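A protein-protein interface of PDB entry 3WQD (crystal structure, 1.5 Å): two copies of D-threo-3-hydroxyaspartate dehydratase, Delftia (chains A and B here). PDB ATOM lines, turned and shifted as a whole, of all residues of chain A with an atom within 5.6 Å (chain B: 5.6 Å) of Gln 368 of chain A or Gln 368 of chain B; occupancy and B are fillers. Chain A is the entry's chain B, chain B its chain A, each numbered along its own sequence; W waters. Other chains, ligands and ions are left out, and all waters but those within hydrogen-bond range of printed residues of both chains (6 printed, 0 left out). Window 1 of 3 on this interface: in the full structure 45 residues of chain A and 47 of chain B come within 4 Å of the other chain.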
ATOM      1  N   TRP A 290      33.841  24.719 -34.742  1.00  0.00           N
ATOM      2  CA  TRP A 290      32.601  23.943 -34.555  1.00  0.00           C
ATOM      3  C   TRP A 290      32.392  23.651 -33.070  1.00  0.00           C
ATOM      4  O   TRP A 290      31.222  23.413 -32.648  1.00  0.00           O
ATOM      5  CB  TRP A 290      32.493  22.687 -35.377  1.00  0.00           C
ATOM      6  CG  TRP A 290      33.542  21.661 -35.144  1.00  0.00           C
ATOM      7  CD1 TRP A 290      34.583  21.345 -36.022  1.00  0.00           C
ATOM      8  CD2 TRP A 290      33.713  20.775 -33.947  1.00  0.00           C
ATOM      9  NE1 TRP A 290      35.411  20.396 -35.459  1.00  0.00           N
ATOM     10  CE2 TRP A 290      34.919  20.028 -34.185  1.00  0.00           C
ATOM     11  CE3 TRP A 290      32.995  20.574 -32.736  1.00  0.00           C
ATOM     12  CZ2 TRP A 290      35.400  19.067 -33.277  1.00  0.00           C
ATOM     13  CZ3 TRP A 290      33.469  19.640 -31.827  1.00  0.00           C
ATOM     14  CH2 TRP A 290      34.671  18.886 -32.083  1.00  0.00           C
ATOM     15  N   MET A 291      33.423  23.747 -32.204  1.00  0.00           N
ATOM     16  CA  MET A 291      33.081  23.581 -30.766  1.00  0.00           C
ATOM     17  C   MET A 291      32.166  24.728 -30.300  1.00  0.00           C
ATOM     18  O   MET A 291      31.354  24.534 -29.399  1.00  0.00           O
ATOM     19  CB  MET A 291      34.361  23.478 -29.929  1.00  0.00           C
ATOM     20  CG  MET A 291      34.067  23.085 -28.432  1.00  0.00           C
ATOM     21  SD  MET A 291      33.361  21.400 -28.293  1.00  0.00           S
ATOM     22  CE  MET A 291      34.866  20.444 -28.596  1.00  0.00           C
ATOM     23  N   ALA A 292      32.329  25.940 -30.835  1.00  0.00           N
ATOM     24  CA  ALA A 292      31.412  27.031 -30.510  1.00  0.00           C
ATOM     25  C   ALA A 292      30.126  26.951 -31.325  1.00  0.00           C
ATOM     26  O   ALA A 292      29.020  27.134 -30.768  1.00  0.00           O
ATOM     27  CB  ALA A 292      32.138  28.394 -30.756  1.00  0.00           C
ATOM     28  N   MET A 293      30.233  26.794 -32.651  1.00  0.00           N
ATOM     29  CA  MET A 293      29.015  26.874 -33.472  1.00  0.00           C
ATOM     30  C   MET A 293      28.175  25.575 -33.430  1.00  0.00           C
ATOM     31  O   MET A 293      27.004  25.628 -33.822  1.00  0.00           O
ATOM     32  CB  MET A 293      29.395  27.125 -34.942  1.00  0.00           C
ATOM     33  CG  MET A 293      30.129  28.504 -35.155  1.00  0.00           C
ATOM     34  SD  MET A 293      29.459  29.917 -34.258  1.00  0.00           S
ATOM     35  CE  MET A 293      27.776  29.990 -34.971  1.00  0.00           C
ATOM     36  N   SER A 294      28.811  24.463 -33.061  1.00  0.00           N
ATOM     37  CA  SER A 294      28.301  23.118 -33.338  1.00  0.00           C
ATOM     38  C   SER A 294      28.629  22.700 -34.787  1.00  0.00           C
ATOM     39  O   SER A 294      28.854  23.586 -35.663  1.00  0.00           O
ATOM     40  CB  SER A 294      26.837  22.830 -32.980  1.00  0.00           C
ATOM     41  OG  SER A 294      25.996  23.147 -34.111  1.00  0.00           O
ATOM     42  N   ALA A 364      21.332  23.632 -31.415  1.00  0.00           N
ATOM     43  CA  ALA A 364      22.633  22.933 -31.510  1.00  0.00           C
ATOM     44  C   ALA A 364      23.737  23.868 -31.020  1.00  0.00           C
ATOM     45  O   ALA A 364      24.614  23.467 -30.221  1.00  0.00           O
ATOM     46  CB  ALA A 364      22.860  22.522 -32.919  1.00  0.00           C
ATOM     47  N   THR A 365      23.716  25.153 -31.470  1.00  0.00           N
ATOM     48  CA  THR A 365      24.788  26.105 -31.027  1.00  0.00           C
ATOM     49  C   THR A 365      24.667  26.309 -29.529  1.00  0.00           C
ATOM     50  O   THR A 365      25.702  26.299 -28.812  1.00  0.00           O
ATOM     51  CB  THR A 365      24.695  27.442 -31.790  1.00  0.00           C
ATOM     52  OG1 THR A 365      24.913  27.159 -33.181  1.00  0.00           O
ATOM     53  CG2 THR A 365      25.650  28.498 -31.229  1.00  0.00           C
ATOM     54  N   GLY A 366      23.457  26.532 -28.994  1.00  0.00           N
ATOM     55  CA  GLY A 366      23.318  26.848 -27.572  1.00  0.00           C
ATOM     56  C   GLY A 366      23.893  25.751 -26.680  1.00  0.00           C
ATOM     57  O   GLY A 366      24.504  26.011 -25.610  1.00  0.00           O
ATOM     58  N   ALA A 367      23.743  24.507 -27.099  1.00  0.00           N
ATOM     59  CA  ALA A 367      24.157  23.376 -26.286  1.00  0.00           C
ATOM     60  C   ALA A 367      25.686  23.288 -26.131  1.00  0.00           C
ATOM     61  O   ALA A 367      26.216  22.553 -25.276  1.00  0.00           O
ATOM     62  CB  ALA A 367      23.643  22.053 -26.901  1.00  0.00           C
ATOM     63  N   GLN A 368      26.423  24.029 -26.972  1.00  0.00           N
ATOM     64  CA  GLN A 368      27.902  24.025 -26.842  1.00  0.00           C
ATOM     65  C   GLN A 368      28.395  24.911 -25.689  1.00  0.00           C
ATOM     66  O   GLN A 368      29.611  24.861 -25.352  1.00  0.00           O
ATOM     67  CB  GLN A 368      28.536  24.525 -28.149  1.00  0.00           C
ATOM     68  CG  GLN A 368      28.152  23.662 -29.360  1.00  0.00           C
ATOM     69  CD  GLN A 368      28.612  22.224 -29.182  1.00  0.00           C
ATOM     70  OE1 GLN A 368      27.837  21.381 -28.682  1.00  0.00           O
ATOM     71  NE2 GLN A 368      29.874  21.938 -29.568  1.00  0.00           N
ATOM     72  N   PHE A 369      27.485  25.661 -25.057  1.00  0.00           N
ATOM     73  CA  PHE A 369      27.911  26.654 -24.037  1.00  0.00           C
ATOM     74  C   PHE A 369      27.386  26.267 -22.666  1.00  0.00           C
ATOM     75  O   PHE A 369      26.195  25.968 -22.526  1.00  0.00           O
ATOM     76  CB  PHE A 369      27.440  28.088 -24.404  1.00  0.00           C
ATOM     77  CG  PHE A 369      28.127  28.584 -25.625  1.00  0.00           C
ATOM     78  CD1 PHE A 369      27.673  28.234 -26.893  1.00  0.00           C
ATOM     79  CD2 PHE A 369      29.323  29.342 -25.515  1.00  0.00           C
ATOM     80  CE1 PHE A 369      28.347  28.699 -28.041  1.00  0.00           C
ATOM     81  CE2 PHE A 369      30.013  29.769 -26.643  1.00  0.00           C
ATOM     82  CZ  PHE A 369      29.522  29.475 -27.914  1.00  0.00           C
ATOM     83  N   PRO A 370      28.230  26.430 -21.604  1.00  0.00           N
ATOM     84  CA  PRO A 370      27.719  26.252 -20.217  1.00  0.00           C
ATOM     85  C   PRO A 370      26.658  27.325 -19.888  1.00  0.00           C
ATOM     86  O   PRO A 370      25.837  27.104 -19.007  1.00  0.00           O
ATOM     87  CB  PRO A 370      28.974  26.441 -19.338  1.00  0.00           C
ATOM     88  CG  PRO A 370      30.118  26.073 -20.258  1.00  0.00           C
ATOM     89  CD  PRO A 370      29.736  26.495 -21.633  1.00  0.00           C
ATOM     90  N   HIS A 388      23.633  21.092 -19.414  1.00  0.00           N
ATOM     91  CA  HIS A 388      24.426  20.232 -20.301  1.00  0.00           C
ATOM     92  C   HIS A 388      24.307  18.785 -19.823  1.00  0.00           C
ATOM     93  O   HIS A 388      24.379  18.498 -18.627  1.00  0.00           O
ATOM     94  CB  HIS A 388      25.905  20.662 -20.159  1.00  0.00           C
ATOM     95  CG  HIS A 388      26.798  19.968 -21.137  1.00  0.00           C
ATOM     96  ND1 HIS A 388      27.994  19.377 -20.756  1.00  0.00           N
ATOM     97  CD2 HIS A 388      26.667  19.770 -22.499  1.00  0.00           C
ATOM     98  CE1 HIS A 388      28.650  18.910 -21.870  1.00  0.00           C
ATOM     99  NE2 HIS A 388      27.822  19.160 -22.954  1.00  0.00           N
ATOM    100  N   GLY A 389      24.016  17.881 -20.763  1.00  0.00           N
ATOM    101  CA  GLY A 389      24.014  16.465 -20.462  1.00  0.00           C
ATOM    102  C   GLY A 389      22.649  15.931 -20.038  1.00  0.00           C
ATOM    103  O   GLY A 389      21.613  16.515 -20.434  1.00  0.00           O
ATOM    104  N   TRP A 390      22.640  14.852 -19.288  1.00  0.00           N
ATOM    105  CA  TRP A 390      21.403  14.092 -18.971  1.00  0.00           C
ATOM    106  C   TRP A 390      21.313  13.805 -17.496  1.00  0.00           C
ATOM    107  O   TRP A 390      22.272  14.110 -16.727  1.00  0.00           O
ATOM    108  CB  TRP A 390      21.419  12.736 -19.739  1.00  0.00           C
ATOM    109  CG  TRP A 390      21.307  12.965 -21.223  1.00  0.00           C
ATOM    110  CD1 TRP A 390      20.154  13.013 -21.981  1.00  0.00           C
ATOM    111  CD2 TRP A 390      22.411  13.300 -22.162  1.00  0.00           C
ATOM    112  NE1 TRP A 390      20.451  13.311 -23.299  1.00  0.00           N
ATOM    113  CE2 TRP A 390      21.805  13.516 -23.459  1.00  0.00           C
ATOM    114  CE3 TRP A 390      23.819  13.420 -22.009  1.00  0.00           C
ATOM    115  CZ2 TRP A 390      22.551  13.893 -24.584  1.00  0.00           C
ATOM    116  CZ3 TRP A 390      24.574  13.816 -23.150  1.00  0.00           C
ATOM    117  CH2 TRP A 390      23.955  14.054 -24.399  1.00  0.00           C
ATOM    118  OXT TRP A 390      20.331  13.167 -17.073  1.00  0.00           O
ATOM    119  N   TRP B 290      21.381  13.669 -32.043  1.00  0.00           N
ATOM    120  CA  TRP B 290      22.630  14.468 -32.287  1.00  0.00           C
ATOM    121  C   TRP B 290      23.030  15.142 -31.000  1.00  0.00           C
ATOM    122  O   TRP B 290      24.231  15.481 -30.890  1.00  0.00           O
ATOM    123  CB  TRP B 290      22.566  15.422 -33.474  1.00  0.00           C
ATOM    124  CG  TRP B 290      21.506  16.473 -33.359  1.00  0.00           C
ATOM    125  CD1 TRP B 290      20.317  16.577 -34.097  1.00  0.00           C
ATOM    126  CD2 TRP B 290      21.522  17.690 -32.482  1.00  0.00           C
ATOM    127  NE1 TRP B 290      19.623  17.700 -33.738  1.00  0.00           N
ATOM    128  CE2 TRP B 290      20.281  18.413 -32.757  1.00  0.00           C
ATOM    129  CE3 TRP B 290      22.444  18.234 -31.545  1.00  0.00           C
ATOM    130  CZ2 TRP B 290      19.946  19.569 -32.094  1.00  0.00           C
ATOM    131  CZ3 TRP B 290      22.072  19.395 -30.862  1.00  0.00           C
ATOM    132  CH2 TRP B 290      20.830  20.054 -31.124  1.00  0.00           C
ATOM    133  N   MET B 291      22.167  15.352 -29.965  1.00  0.00           N
ATOM    134  CA  MET B 291      22.705  15.927 -28.719  1.00  0.00           C
ATOM    135  C   MET B 291      23.731  14.931 -28.117  1.00  0.00           C
ATOM    136  O   MET B 291      24.661  15.354 -27.407  1.00  0.00           O
ATOM    137  CB  MET B 291      21.588  16.287 -27.748  1.00  0.00           C
ATOM    138  CG  MET B 291      22.083  17.053 -26.541  1.00  0.00           C
ATOM    139  SD  MET B 291      22.763  18.688 -26.981  1.00  0.00           S
ATOM    140  CE  MET B 291      21.221  19.569 -27.302  1.00  0.00           C
ATOM    141  N   ALA B 292      23.555  13.612 -28.297  1.00  0.00           N
ATOM    142  CA  ALA B 292      24.522  12.618 -27.768  1.00  0.00           C
ATOM    143  C   ALA B 292      25.661  12.464 -28.818  1.00  0.00           C
ATOM    144  O   ALA B 292      26.863  12.446 -28.444  1.00  0.00           O
ATOM    145  CB  ALA B 292      23.852  11.282 -27.570  1.00  0.00           C
ATOM    146  N   MET B 293      25.344  12.243 -30.101  1.00  0.00           N
ATOM    147  CA  MET B 293      26.419  11.916 -31.057  1.00  0.00           C
ATOM    148  C   MET B 293      27.200  13.155 -31.531  1.00  0.00           C
ATOM    149  O   MET B 293      28.316  12.957 -32.074  1.00  0.00           O
ATOM    150  CB  MET B 293      25.824  11.228 -32.322  1.00  0.00           C
ATOM    151  CG  MET B 293      25.081   9.930 -32.022  1.00  0.00           C
ATOM    152  SD  MET B 293      25.929   8.781 -30.883  1.00  0.00           S
ATOM    153  CE  MET B 293      27.483   8.489 -31.771  1.00  0.00           C
ATOM    154  N   SER B 294      26.638  14.349 -31.368  1.00  0.00           N
ATOM    155  CA  SER B 294      27.012  15.565 -32.097  1.00  0.00           C
ATOM    156  C   SER B 294      26.424  15.519 -33.513  1.00  0.00           C
ATOM    157  O   SER B 294      26.134  14.448 -34.038  1.00  0.00           O
ATOM    158  CB  SER B 294      28.559  15.897 -32.110  1.00  0.00           C
ATOM    159  OG  SER B 294      29.195  15.231 -33.182  1.00  0.00           O
ATOM    160  N   ARG B 295      26.478  16.685 -34.140  1.00  0.00           N
ATOM    161  CA  ARG B 295      26.073  16.810 -35.577  1.00  0.00           C
ATOM    162  C   ARG B 295      27.233  16.400 -36.485  1.00  0.00           C
ATOM    163  O   ARG B 295      27.055  16.527 -37.716  1.00  0.00           O
ATOM    164  CB  ARG B 295      25.664  18.236 -35.882  1.00  0.00           C
ATOM    165  CG  ARG B 295      24.203  18.498 -35.509  1.00  0.00           C
ATOM    166  CD  ARG B 295      23.252  17.705 -36.442  1.00  0.00           C
ATOM    167  NE  ARG B 295      22.006  18.458 -36.607  1.00  0.00           N
ATOM    168  CZ  ARG B 295      20.890  17.956 -37.141  1.00  0.00           C
ATOM    169  NH1 ARG B 295      20.832  16.700 -37.484  1.00  0.00           N
ATOM    170  NH2 ARG B 295      19.824  18.765 -37.309  1.00  0.00           N
ATOM    171  N   ALA B 364      34.217  15.381 -31.249  1.00  0.00           N
ATOM    172  CA  ALA B 364      32.927  16.060 -31.315  1.00  0.00           C
ATOM    173  C   ALA B 364      31.912  15.343 -30.382  1.00  0.00           C
ATOM    174  O   ALA B 364      31.173  15.967 -29.631  1.00  0.00           O
ATOM    175  CB  ALA B 364      32.398  16.097 -32.752  1.00  0.00           C
ATOM    176  N   THR B 365      31.895  13.990 -30.490  1.00  0.00           N
ATOM    177  CA  THR B 365      30.922  13.256 -29.637  1.00  0.00           C
ATOM    178  C   THR B 365      31.247  13.441 -28.148  1.00  0.00           C
ATOM    179  O   THR B 365      30.362  13.670 -27.313  1.00  0.00           O
ATOM    180  CB  THR B 365      30.988  11.762 -29.988  1.00  0.00           C
ATOM    181  OG1 THR B 365      30.502  11.640 -31.336  1.00  0.00           O
ATOM    182  CG2 THR B 365      30.111  10.908 -29.024  1.00  0.00           C
ATOM    183  N   GLY B 366      32.527  13.370 -27.798  1.00  0.00           N
ATOM    184  CA  GLY B 366      32.955  13.439 -26.371  1.00  0.00           C
ATOM    185  C   GLY B 366      32.471  14.777 -25.779  1.00  0.00           C
ATOM    186  O   GLY B 366      32.044  14.808 -24.599  1.00  0.00           O
ATOM    187  N   ALA B 367      32.560  15.874 -26.559  1.00  0.00           N
ATOM    188  CA  ALA B 367      32.181  17.193 -26.064  1.00  0.00           C
ATOM    189  C   ALA B 367      30.708  17.345 -25.689  1.00  0.00           C
ATOM    190  O   ALA B 367      30.321  18.285 -24.974  1.00  0.00           O
ATOM    191  CB  ALA B 367      32.609  18.281 -27.038  1.00  0.00           C
ATOM    192  N   GLN B 368      29.858  16.398 -26.152  1.00  0.00           N
ATOM    193  CA  GLN B 368      28.443  16.437 -25.783  1.00  0.00           C
ATOM    194  C   GLN B 368      28.163  15.959 -24.358  1.00  0.00           C
ATOM    195  O   GLN B 368      27.025  16.123 -23.871  1.00  0.00           O
ATOM    196  CB  GLN B 368      27.684  15.574 -26.800  1.00  0.00           C
ATOM    197  CG  GLN B 368      27.801  16.089 -28.245  1.00  0.00           C
ATOM    198  CD  GLN B 368      27.392  17.534 -28.413  1.00  0.00           C
ATOM    199  OE1 GLN B 368      28.222  18.439 -28.268  1.00  0.00           O
ATOM    200  NE2 GLN B 368      26.140  17.782 -28.840  1.00  0.00           N
ATOM    201  N   PHE B 369      29.182  15.383 -23.673  1.00  0.00           N
ATOM    202  CA  PHE B 369      28.911  14.724 -22.372  1.00  0.00           C
ATOM    203  C   PHE B 369      29.666  15.432 -21.265  1.00  0.00           C
ATOM    204  O   PHE B 369      30.870  15.751 -21.418  1.00  0.00           O
ATOM    205  CB  PHE B 369      29.373  13.247 -22.408  1.00  0.00           C
ATOM    206  CG  PHE B 369      28.518  12.434 -23.320  1.00  0.00           C
ATOM    207  CD1 PHE B 369      28.794  12.372 -24.660  1.00  0.00           C
ATOM    208  CD2 PHE B 369      27.393  11.749 -22.770  1.00  0.00           C
ATOM    209  CE1 PHE B 369      27.927  11.655 -25.539  1.00  0.00           C
ATOM    210  CE2 PHE B 369      26.543  11.010 -23.665  1.00  0.00           C
ATOM    211  CZ  PHE B 369      26.836  11.009 -25.006  1.00  0.00           C
ATOM    212  N   PRO B 370      28.991  15.583 -20.113  1.00  0.00           N
ATOM    213  CA  PRO B 370      29.708  16.078 -18.915  1.00  0.00           C
ATOM    214  C   PRO B 370      30.836  15.150 -18.479  1.00  0.00           C
ATOM    215  O   PRO B 370      31.756  15.624 -17.765  1.00  0.00           O
ATOM    216  CB  PRO B 370      28.622  16.157 -17.835  1.00  0.00           C
ATOM    217  CG  PRO B 370      27.355  16.366 -18.664  1.00  0.00           C
ATOM    218  CD  PRO B 370      27.508  15.509 -19.889  1.00  0.00           C
ATOM    219  N   HIS B 388      33.779  21.308 -20.316  1.00  0.00           N
ATOM    220  CA  HIS B 388      32.898  21.919 -21.290  1.00  0.00           C
ATOM    221  C   HIS B 388      33.116  23.408 -21.230  1.00  0.00           C
ATOM    222  O   HIS B 388      33.202  23.990 -20.136  1.00  0.00           O
ATOM    223  CB  HIS B 388      31.442  21.580 -20.800  1.00  0.00           C
ATOM    224  CG  HIS B 388      30.367  22.027 -21.733  1.00  0.00           C
ATOM    225  ND1 HIS B 388      29.209  22.659 -21.277  1.00  0.00           N
ATOM    226  CD2 HIS B 388      30.224  21.815 -23.087  1.00  0.00           C
ATOM    227  CE1 HIS B 388      28.388  22.875 -22.361  1.00  0.00           C
ATOM    228  NE2 HIS B 388      28.987  22.276 -23.464  1.00  0.00           N
ATOM    229  N   GLY B 389      33.155  24.043 -22.389  1.00  0.00           N
ATOM    230  CA  GLY B 389      33.145  25.509 -22.501  1.00  0.00           C
ATOM    231  C   GLY B 389      34.546  26.137 -22.477  1.00  0.00           C
ATOM    232  O   GLY B 389      35.492  25.486 -22.910  1.00  0.00           O
ATOM    233  N   TRP B 390      34.630  27.407 -22.126  1.00  0.00           N
ATOM    234  CA  TRP B 390      35.836  28.239 -22.243  1.00  0.00           C
ATOM    235  C   TRP B 390      36.089  28.973 -20.992  1.00  0.00           C
ATOM    236  O   TRP B 390      35.230  29.055 -20.081  1.00  0.00           O
ATOM    237  CB  TRP B 390      35.658  29.241 -23.435  1.00  0.00           C
ATOM    238  CG  TRP B 390      35.542  28.546 -24.772  1.00  0.00           C
ATOM    239  CD1 TRP B 390      36.526  28.283 -25.653  1.00  0.00           C
ATOM    240  CD2 TRP B 390      34.335  27.948 -25.325  1.00  0.00           C
ATOM    241  NE1 TRP B 390      36.085  27.554 -26.723  1.00  0.00           N
ATOM    242  CE2 TRP B 390      34.737  27.325 -26.586  1.00  0.00           C
ATOM    243  CE3 TRP B 390      32.981  27.887 -24.916  1.00  0.00           C
ATOM    244  CZ2 TRP B 390      33.805  26.676 -27.428  1.00  0.00           C
ATOM    245  CZ3 TRP B 390      32.091  27.177 -25.730  1.00  0.00           C
ATOM    246  CH2 TRP B 390      32.476  26.579 -26.950  1.00  0.00           C
ATOM    247  OXT TRP B 390      37.187  29.554 -20.899  1.00  0.00           O
HETATM  248  O   HOH W   1      26.805  19.706 -25.705  1.00  0.00           O
HETATM  249  O   HOH W   2      33.425  23.160 -24.998  1.00  0.00           O
HETATM  250  O   HOH W   3      30.368  18.649 -29.936  1.00  0.00           O
HETATM  251  O   HOH W   4      29.635  20.815 -26.099  1.00  0.00           O
HETATM  252  O   HOH W   5      25.397  20.806 -29.867  1.00  0.00           O
HETATM  253  O   HOH W   6      23.239  18.019 -23.432  1.00  0.00           O
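Water W3 lies within hydrogen-bond range of OE1 of Gln 368 of chain B (2.7 Å), O of Ala 364 of chain B (2.8 Å) and NE2 of Gln 368 of chain A (3.3 Å). Water W2 bridges N of Gly 389 of chain B and SD of Met 291 of chain A. Water W5 lies within hydrogen-bond range of OE1 of Gln 368 of chain A (2.8 Å), O of Ala 364 of chain A (2.8 Å) and NE2 of Gln 368 of chain B (3.3 Å). Water W6 bridges N of Gly 389 of chain A (2.8 Å) and SD of Met 291 of chain B (3.6 Å). Water W4 lies within hydrogen-bond range of O of Ala 367 of chain B (2.9 Å), NE2 of His 388 of chain B (3.1 Å) and OE1 of Gln 368 of chain A (3.2 Å). Water W1 lies within hydrogen-bond range of O of Ala 367 of chain A (2.9 Å), NE2 of His 388 of chain A (3.0 Å) and OE1 of Gln 368 of chain B (3.2 Å).
Trp 290 of chain A touches Ala 364 of chain B, and with the chains exchanged Ala 364 of chain A touches Trp 290 of chain B. Met 291 of chain A touches Ala 367 of chain B, and with the chains exchanged Ala 367 of chain A touches Met 291 of chain B. Gln 368 of chain A touches its own counterpart, Gln 368 of chain B. Pro 370 of chain A touches His 388 of chain B, and with the chains exchanged His 388 of chain A touches Pro 370 of chain B. 15 positions are printed for both chains. Of the 24 pairs that touch across the chains among the printed residues, 24 have their exchanged pair printed and touching as well.
Among the printed residues, merely in contact across the chains: Trp 390 of chain A with Met 291 of chain B (3.4 Å), Met 291 of chain A with Trp 390 of chain B (3.4 Å), Trp 290 of chain A with Ala 364 of chain B (3.4 Å), Gln 368 of chain A with Trp 390 of chain B (3.4 Å), Ala 364 of chain A with Trp 290 of chain B (3.4 Å), Trp 390 of chain A with Gln 368 of chain B (3.4 Å), Met 291 of chain A with Ala 367 of chain B (3.4 Å), Phe 369 of chain A with Trp 390 of chain B (3.4 Å), Trp 390 of chain A with Phe 369 of chain B (3.5 Å), Ala 367 of chain A with Met 291 of chain B (3.5 Å), Phe 369 of chain A with His 388 of chain B (3.6 Å), Pro 370 of chain A with His 388 of chain B (3.6 Å), Pro 370 of chain A with Gly 389 of chain B (3.7 Å), His 388 of chain A with Pro 370 of chain B (3.7 Å), Gly 389 of chain A with Pro 370 of chain B (3.7 Å), His 388 of chain A with Phe 369 of chain B (3.7 Å), Trp 390 of chain A with Ala 292 of chain B (3.7 Å) and Ala 292 of chain A with Trp 390 of chain B (3.7 Å).
NE2 of His 388 of chain B is in hydrogen-bond range of O of Gln 368 of chain A (3.3 Å). O of Ala 367 of chain B sits at hydrogen-bond distance from NE2 of His 388 of chain A, 3.3 Å away. A ring nitrogen (NE2) of His 388 of chain B is in hydrogen-bond range of a ring nitrogen (NE2) of His 388 of chain A, at 3.4 Å. A ring nitrogen (NE2) of His 388 of chain B lies within hydrogen-bond range of the backbone carbonyl oxygen (O) of Ala 367 of chain A (3.3 Å). OE1 of Gln 368 of chain B lies close to OE1 of Gln 368 of chain A, 3.0 Å away. NE2 of His 388 of chain A lies within hydrogen-bond range of O of Gln 368 of chain B.
Hydrophobic or aromatic side chains of chain B within 4 Å of the printed part of chain A: Trp 290, Met 291, Ala 364, Ala 367, Phe 369, Pro 370, His 388 and Trp 390. Hydrophobic or aromatic side chains of chain A that line the printed part of chain B: Trp 290, Met 291, Ala 364, Ala 367, Phe 369, Pro 370, His 388 and Trp 390. Along chain A the printed residues that touch a printed residue of chain B span positions 290 to 390. Among the printed residues, 24 pairs touch across the chains.
The side-chain amide nitrogen (NE2) of Gln 368 of chain B lies close to the backbone carbonyl oxygen (O) of Met 291 of chain B, at 3.2 Å. The side-chain amide nitrogen of Gln 368 of chain A is in hydrogen-bond range of the backbone carbonyl oxygen of Met 291 of chain A, 3.0 Å away.
Of the printed residues of chain B, Gln 368 of chain A touches Gln 368, His 388 and Trp 390. Of the printed residues of chain B, His 388 of chain A touches Ala 367 (3.3 Å), Gln 368 (3.3 Å), Phe 369 (3.7 Å), Pro 370 (3.7 Å) and His 388 (3.4 Å). Of the printed residues of chain A, Met 291 of chain B touches Ala 367 (3.5 Å) and Trp 390 (3.4 Å). Printed residues of chain A within 4 Å of Ala 367 of chain B: Met 291 and His 388. Printed residues of chain A within 4 Å of Gln 368 of chain B: Gln 368, His 388 and Trp 390. Of the printed residues of chain A, Gly 389 of chain B touches Pro 370 (3.7 Å).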
